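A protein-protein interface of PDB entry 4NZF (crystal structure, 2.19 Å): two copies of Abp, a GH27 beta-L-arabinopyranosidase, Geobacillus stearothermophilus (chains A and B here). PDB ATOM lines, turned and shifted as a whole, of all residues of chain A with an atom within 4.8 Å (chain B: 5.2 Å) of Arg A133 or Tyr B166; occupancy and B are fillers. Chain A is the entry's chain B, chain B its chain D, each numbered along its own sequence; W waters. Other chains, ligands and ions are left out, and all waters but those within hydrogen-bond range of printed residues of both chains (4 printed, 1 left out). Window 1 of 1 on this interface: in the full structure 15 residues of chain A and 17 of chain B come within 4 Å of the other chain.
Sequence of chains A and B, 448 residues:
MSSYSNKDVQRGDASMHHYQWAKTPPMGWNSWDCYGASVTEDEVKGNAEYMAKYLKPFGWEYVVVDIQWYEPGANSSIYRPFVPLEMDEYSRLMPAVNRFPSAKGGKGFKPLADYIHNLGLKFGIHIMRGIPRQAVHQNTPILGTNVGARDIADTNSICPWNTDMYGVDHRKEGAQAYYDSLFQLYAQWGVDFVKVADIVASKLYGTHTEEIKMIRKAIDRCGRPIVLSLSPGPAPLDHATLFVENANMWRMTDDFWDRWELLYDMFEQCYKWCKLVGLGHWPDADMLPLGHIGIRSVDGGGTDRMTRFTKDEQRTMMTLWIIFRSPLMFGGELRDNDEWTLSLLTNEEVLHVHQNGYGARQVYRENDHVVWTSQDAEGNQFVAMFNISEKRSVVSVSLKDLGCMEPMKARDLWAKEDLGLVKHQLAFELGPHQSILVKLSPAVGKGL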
ATOM      1  N   PHE A  82     -11.803  31.623 -10.213  1.00  0.00           N
ATOM      2  CA  PHE A  82     -11.411  30.739 -11.248  1.00  0.00           C
ATOM      3  C   PHE A  82     -10.085  31.087 -11.922  1.00  0.00           C
ATOM      4  O   PHE A  82      -9.869  30.664 -13.057  1.00  0.00           O
ATOM      5  CB  PHE A  82     -12.548  30.600 -12.294  1.00  0.00           C
ATOM      6  CG  PHE A  82     -13.909  30.286 -11.716  1.00  0.00           C
ATOM      7  CD1 PHE A  82     -14.188  29.020 -11.186  1.00  0.00           C
ATOM      8  CD2 PHE A  82     -14.922  31.218 -11.735  1.00  0.00           C
ATOM      9  CE1 PHE A  82     -15.434  28.735 -10.698  1.00  0.00           C
ATOM     10  CE2 PHE A  82     -16.178  30.906 -11.272  1.00  0.00           C
ATOM     11  CZ  PHE A  82     -16.405  29.696 -10.724  1.00  0.00           C
ATOM     12  N   ILE A 131      -7.610  20.566  -2.442  1.00  0.00           N
ATOM     13  CA  ILE A 131      -6.591  20.426  -3.471  1.00  0.00           C
ATOM     14  C   ILE A 131      -6.993  21.330  -4.598  1.00  0.00           C
ATOM     15  O   ILE A 131      -8.184  21.529  -4.811  1.00  0.00           O
ATOM     16  CB  ILE A 131      -6.383  18.969  -3.895  1.00  0.00           C
ATOM     17  CG1 ILE A 131      -5.231  18.904  -4.865  1.00  0.00           C
ATOM     18  CG2 ILE A 131      -7.630  18.347  -4.507  1.00  0.00           C
ATOM     19  CD1 ILE A 131      -4.730  17.498  -5.075  1.00  0.00           C
ATOM     20  N   PRO A 132      -6.027  21.963  -5.259  1.00  0.00           N
ATOM     21  CA  PRO A 132      -6.465  22.977  -6.217  1.00  0.00           C
ATOM     22  C   PRO A 132      -7.330  22.429  -7.340  1.00  0.00           C
ATOM     23  O   PRO A 132      -7.058  21.349  -7.852  1.00  0.00           O
ATOM     24  CB  PRO A 132      -5.138  23.483  -6.808  1.00  0.00           C
ATOM     25  CG  PRO A 132      -4.164  23.285  -5.735  1.00  0.00           C
ATOM     26  CD  PRO A 132      -4.557  21.992  -5.092  1.00  0.00           C
ATOM     27  N   ARG A 133      -8.360  23.154  -7.697  1.00  0.00           N
ATOM     28  CA  ARG A 133      -9.200  22.720  -8.806  1.00  0.00           C
ATOM     29  C   ARG A 133      -8.363  22.497 -10.108  1.00  0.00           C
ATOM     30  O   ARG A 133      -8.540  21.525 -10.865  1.00  0.00           O
ATOM     31  CB  ARG A 133     -10.283  23.778  -9.034  1.00  0.00           C
ATOM     32  CG  ARG A 133     -11.290  23.900  -7.877  1.00  0.00           C
ATOM     33  CD  ARG A 133     -12.530  24.652  -8.279  1.00  0.00           C
ATOM     34  NE  ARG A 133     -13.422  24.902  -7.154  1.00  0.00           N
ATOM     35  CZ  ARG A 133     -14.578  25.552  -7.234  1.00  0.00           C
ATOM     36  NH1 ARG A 133     -15.111  25.878  -8.404  1.00  0.00           N
ATOM     37  NH2 ARG A 133     -15.248  25.828  -6.142  1.00  0.00           N
ATOM     38  N   GLN A 134      -7.433  23.399 -10.349  1.00  0.00           N
ATOM     39  CA  GLN A 134      -6.604  23.341 -11.560  1.00  0.00           C
ATOM     40  C   GLN A 134      -5.802  22.062 -11.548  1.00  0.00           C
ATOM     41  O   GLN A 134      -5.610  21.451 -12.600  1.00  0.00           O
ATOM     42  CB  GLN A 134      -5.766  24.597 -11.689  1.00  0.00           C
ATOM     43  CG  GLN A 134      -4.734  24.706 -10.593  1.00  0.00           C
ATOM     44  CD  GLN A 134      -3.813  25.900 -10.740  1.00  0.00           C
ATOM     45  OE1 GLN A 134      -4.191  26.965 -11.208  1.00  0.00           O
ATOM     46  NE2 GLN A 134      -2.619  25.740 -10.229  1.00  0.00           N
ATOM     47  N   ALA A 135      -5.457  21.540 -10.371  1.00  0.00           N
ATOM     48  CA  ALA A 135      -4.701  20.289 -10.318  1.00  0.00           C
ATOM     49  C   ALA A 135      -5.529  19.092 -10.686  1.00  0.00           C
ATOM     50  O   ALA A 135      -5.059  18.076 -11.271  1.00  0.00           O
ATOM     51  CB  ALA A 135      -4.065  20.105  -8.956  1.00  0.00           C
ATOM     52  N   VAL A 136      -6.809  19.207 -10.354  1.00  0.00           N
ATOM     53  CA  VAL A 136      -7.717  18.130 -10.622  1.00  0.00           C
ATOM     54  C   VAL A 136      -8.028  18.194 -12.085  1.00  0.00           C
ATOM     55  O   VAL A 136      -8.020  17.197 -12.758  1.00  0.00           O
ATOM     56  CB  VAL A 136      -8.981  18.276  -9.785  1.00  0.00           C
ATOM     57  CG1 VAL A 136     -10.069  17.333 -10.306  1.00  0.00           C
ATOM     58  CG2 VAL A 136      -8.675  17.946  -8.301  1.00  0.00           C
ATOM     59  N   HIS A 137      -8.284  19.377 -12.586  1.00  0.00           N
ATOM     60  CA  HIS A 137      -8.565  19.507 -14.011  1.00  0.00           C
ATOM     61  C   HIS A 137      -7.427  19.032 -14.926  1.00  0.00           C
ATOM     62  O   HIS A 137      -7.681  18.367 -15.954  1.00  0.00           O
ATOM     63  CB  HIS A 137      -8.950  20.948 -14.308  1.00  0.00           C
ATOM     64  CG  HIS A 137     -10.144  21.389 -13.529  1.00  0.00           C
ATOM     65  ND1 HIS A 137     -10.430  22.714 -13.272  1.00  0.00           N
ATOM     66  CD2 HIS A 137     -11.102  20.662 -12.906  1.00  0.00           C
ATOM     67  CE1 HIS A 137     -11.523  22.786 -12.530  1.00  0.00           C
ATOM     68  NE2 HIS A 137     -11.943  21.556 -12.297  1.00  0.00           N
ATOM     69  N   ILE A 158     -16.921  21.727  -2.342  1.00  0.00           N
ATOM     70  CA  ILE A 158     -16.350  22.980  -2.663  1.00  0.00           C
ATOM     71  C   ILE A 158     -16.500  23.921  -1.469  1.00  0.00           C
ATOM     72  O   ILE A 158     -17.160  23.584  -0.483  1.00  0.00           O
ATOM     73  CB  ILE A 158     -17.042  23.680  -3.888  1.00  0.00           C
ATOM     74  CG1 ILE A 158     -18.540  23.935  -3.630  1.00  0.00           C
ATOM     75  CG2 ILE A 158     -16.810  22.900  -5.152  1.00  0.00           C
ATOM     76  CD1 ILE A 158     -19.134  24.992  -4.553  1.00  0.00           C
ATOM     77  N   CYS A 159     -15.900  25.112  -1.580  1.00  0.00           N
ATOM     78  CA  CYS A 159     -15.981  26.115  -0.506  1.00  0.00           C
ATOM     79  C   CYS A 159     -16.908  27.131  -1.121  1.00  0.00           C
ATOM     80  O   CYS A 159     -16.782  27.419  -2.283  1.00  0.00           O
ATOM     81  CB  CYS A 159     -14.607  26.791  -0.161  1.00  0.00           C
ATOM     82  SG  CYS A 159     -14.855  28.359   0.685  1.00  0.00           S
ATOM     83  N   ASN A 162     -15.052  30.724  -1.781  1.00  0.00           N
ATOM     84  CA  ASN A 162     -13.832  30.775  -2.590  1.00  0.00           C
ATOM     85  C   ASN A 162     -13.714  29.602  -3.537  1.00  0.00           C
ATOM     86  O   ASN A 162     -13.998  28.448  -3.157  1.00  0.00           O
ATOM     87  CB  ASN A 162     -12.627  30.835  -1.622  1.00  0.00           C
ATOM     88  CG  ASN A 162     -11.288  30.543  -2.264  1.00  0.00           C
ATOM     89  OD1 ASN A 162     -10.903  29.392  -2.508  1.00  0.00           O
ATOM     90  ND2 ASN A 162     -10.520  31.568  -2.394  1.00  0.00           N
ATOM     91  N   THR A 163     -13.175  29.879  -4.721  1.00  0.00           N
ATOM     92  CA  THR A 163     -13.149  28.899  -5.804  1.00  0.00           C
ATOM     93  C   THR A 163     -11.877  28.111  -6.043  1.00  0.00           C
ATOM     94  O   THR A 163     -11.814  27.415  -7.036  1.00  0.00           O
ATOM     95  CB  THR A 163     -13.447  29.550  -7.165  1.00  0.00           C
ATOM     96  OG1 THR A 163     -12.511  30.578  -7.440  1.00  0.00           O
ATOM     97  CG2 THR A 163     -14.856  30.126  -7.178  1.00  0.00           C
ATOM     98  N   ASP A 164     -10.899  28.174  -5.133  1.00  0.00           N
ATOM     99  CA  ASP A 164      -9.527  27.742  -5.447  1.00  0.00           C
ATOM    100  C   ASP A 164      -9.414  26.231  -5.459  1.00  0.00           C
ATOM    101  O   ASP A 164      -8.661  25.618  -6.254  1.00  0.00           O
ATOM    102  CB  ASP A 164      -8.499  28.434  -4.491  1.00  0.00           C
ATOM    103  CG  ASP A 164      -8.378  29.897  -4.726  1.00  0.00           C
ATOM    104  OD1 ASP A 164      -8.771  30.395  -5.864  1.00  0.00           O
ATOM    105  OD2 ASP A 164      -7.983  30.607  -3.759  1.00  0.00           O
ATOM    106  N   MET A 165     -10.173  25.580  -4.583  1.00  0.00           N
ATOM    107  CA  MET A 165      -9.944  24.159  -4.341  1.00  0.00           C
ATOM    108  C   MET A 165     -11.185  23.299  -4.540  1.00  0.00           C
ATOM    109  O   MET A 165     -12.299  23.781  -4.518  1.00  0.00           O
ATOM    110  CB  MET A 165      -9.525  23.965  -2.879  1.00  0.00           C
ATOM    111  CG  MET A 165      -8.627  24.998  -2.279  1.00  0.00           C
ATOM    112  SD  MET A 165      -6.964  25.081  -3.075  1.00  0.00           S
ATOM    113  CE  MET A 165      -6.000  24.015  -2.050  1.00  0.00           C
ATOM    114  N   TYR A 166     -10.946  22.004  -4.634  1.00  0.00           N
ATOM    115  CA  TYR A 166     -11.909  20.967  -4.359  1.00  0.00           C
ATOM    116  C   TYR A 166     -11.475  20.254  -3.106  1.00  0.00           C
ATOM    117  O   TYR A 166     -10.278  20.183  -2.763  1.00  0.00           O
ATOM    118  CB  TYR A 166     -11.968  19.885  -5.456  1.00  0.00           C
ATOM    119  CG  TYR A 166     -12.498  20.367  -6.790  1.00  0.00           C
ATOM    120  CD1 TYR A 166     -13.718  21.062  -6.889  1.00  0.00           C
ATOM    121  CD2 TYR A 166     -11.772  20.142  -7.957  1.00  0.00           C
ATOM    122  CE1 TYR A 166     -14.176  21.531  -8.126  1.00  0.00           C
ATOM    123  CE2 TYR A 166     -12.244  20.570  -9.204  1.00  0.00           C
ATOM    124  CZ  TYR A 166     -13.423  21.282  -9.294  1.00  0.00           C
ATOM    125  OH  TYR A 166     -13.840  21.747 -10.540  1.00  0.00           O
ATOM    126  N   ARG B 129     -27.840  22.117 -16.660  1.00  0.00           N
ATOM    127  CA  ARG B 129     -27.856  23.489 -16.325  1.00  0.00           C
ATOM    128  C   ARG B 129     -26.433  24.005 -16.277  1.00  0.00           C
ATOM    129  O   ARG B 129     -25.545  23.348 -15.701  1.00  0.00           O
ATOM    130  CB  ARG B 129     -28.477  23.702 -14.957  1.00  0.00           C
ATOM    131  CG  ARG B 129     -28.486  25.154 -14.493  1.00  0.00           C
ATOM    132  CD  ARG B 129     -28.874  25.152 -13.024  1.00  0.00           C
ATOM    133  NE  ARG B 129     -27.929  24.420 -12.163  1.00  0.00           N
ATOM    134  CZ  ARG B 129     -27.097  25.021 -11.281  1.00  0.00           C
ATOM    135  NH1 ARG B 129     -27.031  26.342 -11.177  1.00  0.00           N
ATOM    136  NH2 ARG B 129     -26.305  24.301 -10.490  1.00  0.00           N
ATOM    137  N   GLY B 130     -26.250  25.179 -16.864  1.00  0.00           N
ATOM    138  CA  GLY B 130     -25.035  25.959 -16.651  1.00  0.00           C
ATOM    139  C   GLY B 130     -24.079  26.034 -17.826  1.00  0.00           C
ATOM    140  O   GLY B 130     -24.492  25.927 -18.990  1.00  0.00           O
ATOM    141  N   ILE B 131     -22.811  26.313 -17.525  1.00  0.00           N
ATOM    142  CA  ILE B 131     -21.750  26.434 -18.534  1.00  0.00           C
ATOM    143  C   ILE B 131     -20.607  25.505 -18.168  1.00  0.00           C
ATOM    144  O   ILE B 131     -20.359  25.297 -17.025  1.00  0.00           O
ATOM    145  CB  ILE B 131     -21.271  27.857 -18.611  1.00  0.00           C
ATOM    146  CG1 ILE B 131     -20.284  28.076 -19.773  1.00  0.00           C
ATOM    147  CG2 ILE B 131     -20.666  28.245 -17.269  1.00  0.00           C
ATOM    148  CD1 ILE B 131     -20.100  29.543 -20.223  1.00  0.00           C
ATOM    149  N   PRO B 132     -19.931  24.891 -19.140  1.00  0.00           N
ATOM    150  CA  PRO B 132     -19.012  23.837 -18.691  1.00  0.00           C
ATOM    151  C   PRO B 132     -17.822  24.362 -17.844  1.00  0.00           C
ATOM    152  O   PRO B 132     -17.340  25.490 -18.007  1.00  0.00           O
ATOM    153  CB  PRO B 132     -18.490  23.282 -20.000  1.00  0.00           C
ATOM    154  CG  PRO B 132     -19.643  23.498 -20.969  1.00  0.00           C
ATOM    155  CD  PRO B 132     -20.123  24.875 -20.604  1.00  0.00           C
ATOM    156  N   ARG B 133     -17.396  23.565 -16.903  1.00  0.00           N
ATOM    157  CA  ARG B 133     -16.346  24.025 -16.007  1.00  0.00           C
ATOM    158  C   ARG B 133     -15.062  24.248 -16.843  1.00  0.00           C
ATOM    159  O   ARG B 133     -14.399  25.217 -16.624  1.00  0.00           O
ATOM    160  CB  ARG B 133     -16.118  23.005 -14.905  1.00  0.00           C
ATOM    161  CG  ARG B 133     -17.319  22.814 -13.959  1.00  0.00           C
ATOM    162  CD  ARG B 133     -16.861  22.091 -12.694  1.00  0.00           C
ATOM    163  NE  ARG B 133     -17.957  21.684 -11.828  1.00  0.00           N
ATOM    164  CZ  ARG B 133     -17.826  21.006 -10.701  1.00  0.00           C
ATOM    165  NH1 ARG B 133     -16.621  20.736 -10.202  1.00  0.00           N
ATOM    166  NH2 ARG B 133     -18.906  20.649 -10.042  1.00  0.00           N
ATOM    167  N   VAL B 136     -15.120  27.683 -18.154  1.00  0.00           N
ATOM    168  CA  VAL B 136     -14.886  28.722 -17.205  1.00  0.00           C
ATOM    169  C   VAL B 136     -13.403  28.837 -16.818  1.00  0.00           C
ATOM    170  O   VAL B 136     -12.902  29.944 -16.665  1.00  0.00           O
ATOM    171  CB  VAL B 136     -15.809  28.457 -15.993  1.00  0.00           C
ATOM    172  CG1 VAL B 136     -15.332  29.101 -14.702  1.00  0.00           C
ATOM    173  CG2 VAL B 136     -17.227  28.939 -16.365  1.00  0.00           C
ATOM    174  N   HIS B 137     -12.730  27.714 -16.697  1.00  0.00           N
ATOM    175  CA  HIS B 137     -11.366  27.670 -16.243  1.00  0.00           C
ATOM    176  C   HIS B 137     -10.403  28.160 -17.355  1.00  0.00           C
ATOM    177  O   HIS B 137      -9.541  29.009 -17.101  1.00  0.00           O
ATOM    178  CB  HIS B 137     -11.057  26.305 -15.687  1.00  0.00           C
ATOM    179  CG  HIS B 137     -11.598  26.132 -14.301  1.00  0.00           C
ATOM    180  ND1 HIS B 137     -10.939  26.599 -13.181  1.00  0.00           N
ATOM    181  CD2 HIS B 137     -12.792  25.658 -13.858  1.00  0.00           C
ATOM    182  CE1 HIS B 137     -11.682  26.381 -12.108  1.00  0.00           C
ATOM    183  NE2 HIS B 137     -12.815  25.819 -12.493  1.00  0.00           N
ATOM    184  N   ALA B 153     -20.028  32.848 -14.950  1.00  0.00           N
ATOM    185  CA  ALA B 153     -20.152  31.746 -14.039  1.00  0.00           C
ATOM    186  C   ALA B 153     -20.490  32.255 -12.652  1.00  0.00           C
ATOM    187  O   ALA B 153     -20.059  33.325 -12.218  1.00  0.00           O
ATOM    188  CB  ALA B 153     -18.883  30.936 -13.979  1.00  0.00           C
ATOM    189  N   ASP B 154     -21.335  31.462 -12.010  1.00  0.00           N
ATOM    190  CA  ASP B 154     -21.639  31.590 -10.611  1.00  0.00           C
ATOM    191  C   ASP B 154     -20.475  31.059  -9.816  1.00  0.00           C
ATOM    192  O   ASP B 154     -19.944  30.028 -10.156  1.00  0.00           O
ATOM    193  CB  ASP B 154     -22.800  30.693 -10.319  1.00  0.00           C
ATOM    194  CG  ASP B 154     -23.756  31.316  -9.447  1.00  0.00           C
ATOM    195  OD1 ASP B 154     -23.412  31.496  -8.182  1.00  0.00           O
ATOM    196  OD2 ASP B 154     -24.793  31.621 -10.114  1.00  0.00           O
ATOM    197  N   THR B 155     -20.080  31.739  -8.763  1.00  0.00           N
ATOM    198  CA  THR B 155     -18.940  31.271  -8.000  1.00  0.00           C
ATOM    199  C   THR B 155     -19.310  30.205  -6.989  1.00  0.00           C
ATOM    200  O   THR B 155     -18.410  29.488  -6.535  1.00  0.00           O
ATOM    201  CB  THR B 155     -18.257  32.436  -7.305  1.00  0.00           C
ATOM    202  OG1 THR B 155     -19.220  33.144  -6.515  1.00  0.00           O
ATOM    203  CG2 THR B 155     -17.719  33.404  -8.389  1.00  0.00           C
ATOM    204  N   SER B 157     -22.157  27.466  -7.227  1.00  0.00           N
ATOM    205  CA  SER B 157     -23.274  26.784  -7.854  1.00  0.00           C
ATOM    206  C   SER B 157     -22.766  25.719  -8.779  1.00  0.00           C
ATOM    207  O   SER B 157     -22.204  25.974  -9.817  1.00  0.00           O
ATOM    208  CB  SER B 157     -24.184  27.758  -8.586  1.00  0.00           C
ATOM    209  OG  SER B 157     -25.271  27.115  -9.223  1.00  0.00           O
ATOM    210  N   ILE B 158     -22.939  24.508  -8.333  1.00  0.00           N
ATOM    211  CA  ILE B 158     -22.567  23.311  -8.984  1.00  0.00           C
ATOM    212  C   ILE B 158     -23.745  22.344  -8.815  1.00  0.00           C
ATOM    213  O   ILE B 158     -24.715  22.632  -8.100  1.00  0.00           O
ATOM    214  CB  ILE B 158     -21.331  22.647  -8.291  1.00  0.00           C
ATOM    215  CG1 ILE B 158     -21.588  22.395  -6.785  1.00  0.00           C
ATOM    216  CG2 ILE B 158     -20.101  23.541  -8.369  1.00  0.00           C
ATOM    217  CD1 ILE B 158     -20.689  21.306  -6.203  1.00  0.00           C
ATOM    218  N   ASP B 164     -19.808  18.386 -14.467  1.00  0.00           N
ATOM    219  CA  ASP B 164     -19.517  18.889 -15.839  1.00  0.00           C
ATOM    220  C   ASP B 164     -19.598  20.426 -15.928  1.00  0.00           C
ATOM    221  O   ASP B 164     -18.753  21.079 -16.561  1.00  0.00           O
ATOM    222  CB  ASP B 164     -20.410  18.210 -16.895  1.00  0.00           C
ATOM    223  CG  ASP B 164     -20.140  16.721 -17.033  1.00  0.00           C
ATOM    224  OD1 ASP B 164     -19.044  16.179 -16.554  1.00  0.00           O
ATOM    225  OD2 ASP B 164     -21.064  16.034 -17.588  1.00  0.00           O
ATOM    226  N   MET B 165     -20.560  21.019 -15.222  1.00  0.00           N
ATOM    227  CA  MET B 165     -20.829  22.416 -15.336  1.00  0.00           C
ATOM    228  C   MET B 165     -20.651  23.217 -14.041  1.00  0.00           C
ATOM    229  O   MET B 165     -20.589  22.672 -12.930  1.00  0.00           O
ATOM    230  CB  MET B 165     -22.307  22.631 -15.688  1.00  0.00           C
ATOM    231  CG  MET B 165     -22.874  21.689 -16.693  1.00  0.00           C
ATOM    232  SD  MET B 165     -22.084  21.696 -18.314  1.00  0.00           S
ATOM    233  CE  MET B 165     -23.043  22.973 -19.095  1.00  0.00           C
ATOM    234  N   TYR B 166     -20.719  24.519 -14.222  1.00  0.00           N
ATOM    235  CA  TYR B 166     -21.066  25.471 -13.190  1.00  0.00           C
ATOM    236  C   TYR B 166     -22.324  26.194 -13.606  1.00  0.00           C
ATOM    237  O   TYR B 166     -22.608  26.365 -14.767  1.00  0.00           O
ATOM    238  CB  TYR B 166     -20.009  26.586 -12.964  1.00  0.00           C
ATOM    239  CG  TYR B 166     -18.633  26.110 -12.451  1.00  0.00           C
ATOM    240  CD1 TYR B 166     -18.530  25.355 -11.310  1.00  0.00           C
ATOM    241  CD2 TYR B 166     -17.433  26.452 -13.120  1.00  0.00           C
ATOM    242  CE1 TYR B 166     -17.286  24.946 -10.829  1.00  0.00           C
ATOM    243  CE2 TYR B 166     -16.206  26.027 -12.650  1.00  0.00           C
ATOM    244  CZ  TYR B 166     -16.140  25.273 -11.496  1.00  0.00           C
ATOM    245  OH  TYR B 166     -14.958  24.828 -10.980  1.00  0.00           O
ATOM    246  N   GLY B 167     -23.052  26.638 -12.610  1.00  0.00           N
ATOM    247  CA  GLY B 167     -24.174  27.501 -12.818  1.00  0.00           C
ATOM    248  C   GLY B 167     -23.783  28.811 -13.419  1.00  0.00           C
ATOM    249  O   GLY B 167     -22.684  29.338 -13.169  1.00  0.00           O
ATOM    250  N   VAL B 168     -24.734  29.354 -14.168  1.00  0.00           N
ATOM    251  CA  VAL B 168     -24.653  30.692 -14.703  1.00  0.00           C
ATOM    252  C   VAL B 168     -25.451  31.708 -13.924  1.00  0.00           C
ATOM    253  O   VAL B 168     -26.608  31.480 -13.589  1.00  0.00           O
ATOM    254  CB  VAL B 168     -25.217  30.705 -16.147  1.00  0.00           C
ATOM    255  CG1 VAL B 168     -25.353  32.133 -16.694  1.00  0.00           C
ATOM    256  CG2 VAL B 168     -24.404  29.811 -17.033  1.00  0.00           C
HETATM  257  O   HOH W   1     -12.536  22.648 -15.950  1.00  0.00           O
HETATM  258  O   HOH W   2     -17.556  27.206  -7.629  1.00  0.00           O
HETATM  259  O   HOH W   3      -8.201  24.787 -14.115  1.00  0.00           O
HETATM  260  O   HOH W   4      -8.035  29.307 -14.213  1.00  0.00           O
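OH of Tyr B166 is in hydrogen-bond range of NH1 of Arg A133 (2.8 Å).
NH1 of Arg B133 sits at hydrogen-bond distance from OH of Tyr A166 (3.0 Å).
The side-chain hydroxyl (OH) of Tyr B166 is in hydrogen-bond range of the side-chain hydroxyl (OH) of Tyr A166 (3.3 Å).
N of Ile A131 lies within hydrogen-bond range of O of Tyr A166 (2.7 Å).
The backbone carbonyl oxygen of Arg A133 sits close to a ring nitrogen (ND1) of His A137 (3.3 Å).
The backbone NH (N) of Arg A133 sits at hydrogen-bond distance from the backbone carbonyl oxygen (O) of Asp A164 (2.9 Å).
The guanidinium group of Arg A133 is in hydrogen-bond range of the backbone carbonyl oxygen of Met A165, 3.1 Å away.
The backbone NH of Ile B131 sits at hydrogen-bond distance from the backbone carbonyl oxygen of Tyr B166, 2.8 Å away.
A ring nitrogen (NE2) of His B137 sits at hydrogen-bond distance from the side-chain hydroxyl of Tyr B166, 2.8 Å away.
CG of Phe A82 touches CG1 of Val B136, 3.5 Å away.
Phe A82 touches His B137 (CD1 to NE2, 3.7 Å).
CE2 of Phe A82 touches CB of Ala B153, 3.8 Å away.
Asp B154 touches Phe A82 (O to CZ, 3.6 Å).
Phe A82 touches Tyr B166 (CE1 to CE2, 3.4 Å).
His A137 touches His B137 (CE1 to NE2, 3.3 Å).
O of Thr B155 touches CG2 of Thr A163 (3.7 Å).
Printed residues of chain B within 4 Å of Phe A82: Val B136 (3.5 Å), His B137 (3.7 Å), Ala B153 (3.8 Å), Asp B154 (3.6 Å) and Tyr B166 (3.4 Å).
Arg A133 touches just one residue of chain B: Tyr B166.
Of the printed residues of chain B, Tyr A166 touches Arg B133 (3.0 Å) and Tyr B166 (3.3 Å).
Of the printed residues of chain A, Arg B133 touches Tyr A166.
Printed residues of chain A within 4 Å of His B137: Phe A82 and His A137.
Of the printed residues of chain A, Ala B153 touches Phe A82.
Gly B167 touches none of the printed residues of chain A.
Printed residues of chain B that touch a printed residue of chain A: Arg B133, Val B136, His B137, Ala B153, Asp B154, Thr B155 and Tyr B166.
Of the 15 printed residues of chain A, 5 touch a printed residue of chain B.
Printed residues of chain A that touch a printed residue of chain B: Phe A82, Arg A133, His A137, Thr A163 and Tyr A166.
Among the printed residues, 10 pairs touch across the chains.
Among the printed residues, no Asp or Glu carboxylate lies within 4 Å of a Lys or Arg side-chain nitrogen of the other chain.
Arg A133 touches Tyr B166, and with the chains exchanged Tyr A166 touches Arg B133.
His A137 touches its own counterpart, His B137.
Tyr B166 touches its own counterpart, Tyr A166.
Of the 10 pairs that touch across the chains among the printed residues, 4 have their exchanged pair printed and touching as well.
Water W4 bridges the backbone carbonyl oxygen (O) of Phe A82 and the backbone carbonyl oxygen (O) of His B137.
Water W2 lies within hydrogen-bond range of O of Thr B155 (2.7 Å) and NH1 of Arg A133 (2.9 Å).
Water W3 lies within hydrogen-bond range of ND1 of His A137 (3.2 Å) and ND1 of His B137 (3.4 Å).
Water W1 bridges the backbone carbonyl oxygen (O) of Arg B133 (3.2 Å) and a ring nitrogen (ND1) of His A137 (3.4 Å).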
